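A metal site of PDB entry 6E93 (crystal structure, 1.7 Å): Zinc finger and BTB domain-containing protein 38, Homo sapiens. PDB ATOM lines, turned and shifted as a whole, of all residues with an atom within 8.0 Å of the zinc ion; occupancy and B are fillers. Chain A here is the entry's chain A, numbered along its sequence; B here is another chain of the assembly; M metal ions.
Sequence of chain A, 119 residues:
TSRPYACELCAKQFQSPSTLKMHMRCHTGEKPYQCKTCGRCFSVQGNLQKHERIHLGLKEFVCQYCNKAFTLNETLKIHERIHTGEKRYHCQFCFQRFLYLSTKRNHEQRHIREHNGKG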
ATOM      1  N   ALA A   6      -3.942 -17.971  33.441  1.00  0.00           N
ATOM      2  CA  ALA A   6      -2.849 -17.014  33.389  1.00  0.00           C
ATOM      3  C   ALA A   6      -1.580 -17.657  32.830  1.00  0.00           C
ATOM      4  O   ALA A   6      -1.327 -18.849  33.047  1.00  0.00           O
ATOM      5  CB  ALA A   6      -2.563 -16.415  34.779  1.00  0.00           C
ATOM      6  N   CYS A   7      -0.801 -16.859  32.100  1.00  0.00           N
ATOM      7  CA  CYS A   7       0.463 -17.332  31.546  1.00  0.00           C
ATOM      8  C   CYS A   7       1.545 -17.280  32.614  1.00  0.00           C
ATOM      9  O   CYS A   7       1.790 -16.225  33.206  1.00  0.00           O
ATOM     10  CB  CYS A   7       0.875 -16.490  30.338  1.00  0.00           C
ATOM     11  SG  CYS A   7       2.441 -17.029  29.583  1.00  0.00           S
ATOM     12  N   GLU A   8       2.194 -18.426  32.839  1.00  0.00           N
ATOM     13  CA  GLU A   8       3.273 -18.522  33.819  1.00  0.00           C
ATOM     14  C   GLU A   8       4.476 -17.659  33.458  1.00  0.00           C
ATOM     15  O   GLU A   8       5.355 -17.479  34.307  1.00  0.00           O
ATOM     16  CB  GLU A   8       3.732 -19.971  33.963  1.00  0.00           C
ATOM     17  CG  GLU A   8       2.621 -20.988  34.143  1.00  0.00           C
ATOM     18  CD  GLU A   8       2.243 -21.181  35.599  1.00  0.00           C
ATOM     19  OE1 GLU A   8       1.926 -20.180  36.279  1.00  0.00           O
ATOM     20  OE2 GLU A   8       2.263 -22.347  36.070  1.00  0.00           O
ATOM     21  N   LEU A   9       4.543 -17.127  32.244  1.00  0.00           N
ATOM     22  CA  LEU A   9       5.751 -16.470  31.767  1.00  0.00           C
ATOM     23  C   LEU A   9       5.613 -14.969  31.561  1.00  0.00           C
ATOM     24  O   LEU A   9       6.633 -14.282  31.478  1.00  0.00           O
ATOM     25  CB  LEU A   9       6.240 -17.125  30.463  1.00  0.00           C
ATOM     26  CG  LEU A   9       6.515 -18.619  30.569  1.00  0.00           C
ATOM     27  CD1 LEU A   9       7.143 -19.191  29.296  1.00  0.00           C
ATOM     28  CD2 LEU A   9       7.409 -18.909  31.768  1.00  0.00           C
ATOM     29  N   CYS A  10       4.386 -14.433  31.479  1.00  0.00           N
ATOM     30  CA  CYS A  10       4.267 -12.998  31.214  1.00  0.00           C
ATOM     31  C   CYS A  10       3.028 -12.347  31.837  1.00  0.00           C
ATOM     32  O   CYS A  10       2.791 -11.168  31.572  1.00  0.00           O
ATOM     33  CB  CYS A  10       4.275 -12.739  29.699  1.00  0.00           C
ATOM     34  SG  CYS A  10       2.775 -13.233  28.822  1.00  0.00           S
ATOM     35  N   ALA A  11       2.239 -13.066  32.632  1.00  0.00           N
ATOM     36  CA  ALA A  11       1.097 -12.552  33.403  1.00  0.00           C
ATOM     37  C   ALA A  11      -0.132 -12.240  32.570  1.00  0.00           C
ATOM     38  O   ALA A  11      -1.192 -11.993  33.136  1.00  0.00           O
ATOM     39  CB  ALA A  11       1.471 -11.321  34.238  1.00  0.00           C
ATOM     40  N   LYS A  12      -0.039 -12.213  31.229  1.00  0.00           N
ATOM     41  CA  LYS A  12      -1.261 -12.115  30.427  1.00  0.00           C
ATOM     42  C   LYS A  12      -2.231 -13.238  30.806  1.00  0.00           C
ATOM     43  O   LYS A  12      -1.820 -14.323  31.237  1.00  0.00           O
ATOM     44  CB  LYS A  12      -0.935 -12.168  28.934  1.00  0.00           C
ATOM     45  CG  LYS A  12      -0.476 -10.839  28.332  1.00  0.00           C
ATOM     46  CD  LYS A  12      -0.276 -10.973  26.824  1.00  0.00           C
ATOM     47  CE  LYS A  12      -0.032  -9.634  26.141  1.00  0.00           C
ATOM     48  NZ  LYS A  12      -1.209  -9.165  25.335  1.00  0.00           N
ATOM     49  N   GLN A  13      -3.526 -12.981  30.653  1.00  0.00           N
ATOM     50  CA  GLN A  13      -4.560 -13.912  31.094  1.00  0.00           C
ATOM     51  C   GLN A  13      -5.524 -14.219  29.955  1.00  0.00           C
ATOM     52  O   GLN A  13      -5.769 -13.381  29.085  1.00  0.00           O
ATOM     53  CB  GLN A  13      -5.346 -13.374  32.298  1.00  0.00           C
ATOM     54  CG  GLN A  13      -4.605 -13.497  33.609  1.00  0.00           C
ATOM     55  CD  GLN A  13      -5.473 -13.088  34.793  1.00  0.00           C
ATOM     56  OE1 GLN A  13      -6.519 -12.470  34.626  1.00  0.00           O
ATOM     57  NE2 GLN A  13      -5.025 -13.440  35.996  1.00  0.00           N
ATOM     58  N   PHE A  14      -6.090 -15.440  29.987  1.00  0.00           N
ATOM     59  CA  PHE A  14      -6.840 -15.991  28.855  1.00  0.00           C
ATOM     60  C   PHE A  14      -8.071 -16.744  29.341  1.00  0.00           C
ATOM     61  O   PHE A  14      -8.187 -17.100  30.507  1.00  0.00           O
ATOM     62  CB  PHE A  14      -5.931 -16.887  28.002  1.00  0.00           C
ATOM     63  CG  PHE A  14      -4.761 -16.152  27.437  1.00  0.00           C
ATOM     64  CD1 PHE A  14      -4.895 -15.402  26.282  1.00  0.00           C
ATOM     65  CD2 PHE A  14      -3.551 -16.133  28.106  1.00  0.00           C
ATOM     66  CE1 PHE A  14      -3.834 -14.680  25.772  1.00  0.00           C
ATOM     67  CE2 PHE A  14      -2.479 -15.419  27.601  1.00  0.00           C
ATOM     68  CZ  PHE A  14      -2.623 -14.693  26.430  1.00  0.00           C
ATOM     69  N   LEU A  20      -4.941 -20.255  26.042  1.00  0.00           N
ATOM     70  CA  LEU A  20      -3.652 -20.257  26.717  1.00  0.00           C
ATOM     71  C   LEU A  20      -2.629 -21.099  25.951  1.00  0.00           C
ATOM     72  O   LEU A  20      -1.485 -20.672  25.743  1.00  0.00           O
ATOM     73  CB  LEU A  20      -3.796 -20.778  28.146  1.00  0.00           C
ATOM     74  CG  LEU A  20      -2.469 -20.880  28.910  1.00  0.00           C
ATOM     75  CD1 LEU A  20      -1.932 -19.474  29.172  1.00  0.00           C
ATOM     76  CD2 LEU A  20      -2.606 -21.660  30.213  1.00  0.00           C
ATOM     77  N   HIS A  23      -1.402 -19.037  23.148  1.00  0.00           N
ATOM     78  CA  HIS A  23      -0.485 -17.979  23.575  1.00  0.00           C
ATOM     79  C   HIS A  23       0.894 -18.534  23.894  1.00  0.00           C
ATOM     80  O   HIS A  23       1.916 -17.883  23.626  1.00  0.00           O
ATOM     81  CB  HIS A  23      -1.042 -17.253  24.801  1.00  0.00           C
ATOM     82  CG  HIS A  23      -0.057 -16.323  25.421  1.00  0.00           C
ATOM     83  ND1 HIS A  23       0.241 -15.092  24.878  1.00  0.00           N
ATOM     84  CD2 HIS A  23       0.744 -16.455  26.517  1.00  0.00           C
ATOM     85  CE1 HIS A  23       1.158 -14.491  25.627  1.00  0.00           C
ATOM     86  NE2 HIS A  23       1.472 -15.298  26.618  1.00  0.00           N
ATOM     87  N   MET A  24       0.962 -19.718  24.504  1.00  0.00           N
ATOM     88  CA  MET A  24       2.266 -20.262  24.889  1.00  0.00           C
ATOM     89  C   MET A  24       3.164 -20.476  23.685  1.00  0.00           C
ATOM     90  O   MET A  24       4.387 -20.581  23.832  1.00  0.00           O
ATOM     91  CB  MET A  24       2.081 -21.556  25.674  1.00  0.00           C
ATOM     92  CG  MET A  24       1.493 -21.335  27.062  1.00  0.00           C
ATOM     93  SD  MET A  24       2.584 -20.313  28.082  1.00  0.00           S
ATOM     94  CE  MET A  24       4.105 -21.247  27.937  1.00  0.00           C
ATOM     95  N   ARG A  25       2.585 -20.547  22.476  1.00  0.00           N
ATOM     96  CA  ARG A  25       3.419 -20.694  21.290  1.00  0.00           C
ATOM     97  C   ARG A  25       4.243 -19.458  21.021  1.00  0.00           C
ATOM     98  O   ARG A  25       5.270 -19.546  20.334  1.00  0.00           O
ATOM     99  CB  ARG A  25       2.561 -21.043  20.077  1.00  0.00           C
ATOM    100  CG  ARG A  25       1.932 -22.407  20.212  1.00  0.00           C
ATOM    101  CD  ARG A  25       0.985 -22.718  19.073  1.00  0.00           C
ATOM    102  NE  ARG A  25       0.340 -24.003  19.302  1.00  0.00           N
ATOM    103  CZ  ARG A  25      -0.860 -24.336  18.841  1.00  0.00           C
ATOM    104  NH1 ARG A  25      -1.553 -23.470  18.096  1.00  0.00           N
ATOM    105  NH2 ARG A  25      -1.365 -25.529  19.111  1.00  0.00           N
ATOM    106  N   CYS A  26       3.828 -18.298  21.553  1.00  0.00           N
ATOM    107  CA  CYS A  26       4.664 -17.115  21.439  1.00  0.00           C
ATOM    108  C   CYS A  26       5.961 -17.282  22.215  1.00  0.00           C
ATOM    109  O   CYS A  26       6.968 -16.655  21.886  1.00  0.00           O
ATOM    110  CB  CYS A  26       3.927 -15.882  21.964  1.00  0.00           C
ATOM    111  SG  CYS A  26       2.321 -15.635  21.221  1.00  0.00           S
ATOM    112  N   HIS A  27       5.942 -18.111  23.263  1.00  0.00           N
ATOM    113  CA  HIS A  27       7.107 -18.320  24.113  1.00  0.00           C
ATOM    114  C   HIS A  27       7.922 -19.538  23.704  1.00  0.00           C
ATOM    115  O   HIS A  27       9.148 -19.531  23.867  1.00  0.00           O
ATOM    116  CB  HIS A  27       6.700 -18.485  25.577  1.00  0.00           C
ATOM    117  CG  HIS A  27       6.092 -17.246  26.181  1.00  0.00           C
ATOM    118  ND1 HIS A  27       6.775 -16.049  26.263  1.00  0.00           N
ATOM    119  CD2 HIS A  27       4.881 -17.025  26.734  1.00  0.00           C
ATOM    120  CE1 HIS A  27       6.006 -15.150  26.843  1.00  0.00           C
ATOM    121  NE2 HIS A  27       4.853 -15.713  27.138  1.00  0.00           N
ATOM    122  P    DT B  12      -1.078 -12.806  22.369  1.00  0.00           P
ATOM    123  OP1  DT B  12      -0.210 -12.017  23.254  1.00  0.00           O
ATOM    124  OP2  DT B  12      -1.115 -14.276  22.453  1.00  0.00           O
ATOM    125  O5'  DT B  12      -2.583 -12.325  22.577  1.00  0.00           O
ATOM    126  C5'  DT B  12      -2.895 -10.981  22.333  1.00  0.00           C
ATOM    127  C4'  DT B  12      -4.257 -10.832  21.665  1.00  0.00           C
ATOM    128  O4'  DT B  12      -4.255 -11.458  20.378  1.00  0.00           O
ATOM    129  C3'  DT B  12      -5.451 -11.430  22.425  1.00  0.00           C
ATOM    130  O3'  DT B  12      -6.276 -10.365  22.863  1.00  0.00           O
ATOM    131  C2'  DT B  12      -6.161 -12.297  21.368  1.00  0.00           C
ATOM    132  C1'  DT B  12      -5.585 -11.751  20.071  1.00  0.00           C
ATOM    133  N1   DT B  12      -5.612 -12.711  18.921  1.00  0.00           N
ATOM    134  C2   DT B  12      -6.425 -12.451  17.839  1.00  0.00           C
ATOM    135  O2   DT B  12      -7.117 -11.465  17.765  1.00  0.00           O
ATOM    136  N3   DT B  12      -6.379 -13.388  16.845  1.00  0.00           N
ATOM    137  C4   DT B  12      -5.626 -14.531  16.810  1.00  0.00           C
ATOM    138  O4   DT B  12      -5.646 -15.316  15.856  1.00  0.00           O
ATOM    139  C5   DT B  12      -4.791 -14.758  17.973  1.00  0.00           C
ATOM    140  C7   DT B  12      -3.926 -15.986  18.059  1.00  0.00           C
ATOM    141  C6   DT B  12      -4.822 -13.838  18.969  1.00  0.00           C
HETATM  142 ZN    ZN M   1       2.939 -15.359  28.118  1.00  0.00          ZN
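The side-chain sulfur (SG) of Cys 26 sits close to the backbone carbonyl oxygen (O) of His 23.
A ring nitrogen (ND1) of His 23 sits at hydrogen-bond distance from OP2 of DT 12 of chain B (2.9 Å).
SG of Cys 7 lies close to N of Leu 9 (3.4 Å).
The side-chain sulfur of Met 24 lies close to the side-chain sulfur of Cys 7, at 3.6 Å.
The backbone NH of Cys 7 is in hydrogen-bond range of the backbone carbonyl oxygen of Lys 12 of chain A (2.9 Å).
Within 4 Å of the zinc ion: Cys 7, Cys 10, His 23 and His 27.
The zinc ion is bound by NE2 of His 23 (2.1 Å), NE2 of His 27 (2.2 Å), SG of Cys 10 (2.2 Å) and SG of Cys 7 (2.3 Å).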
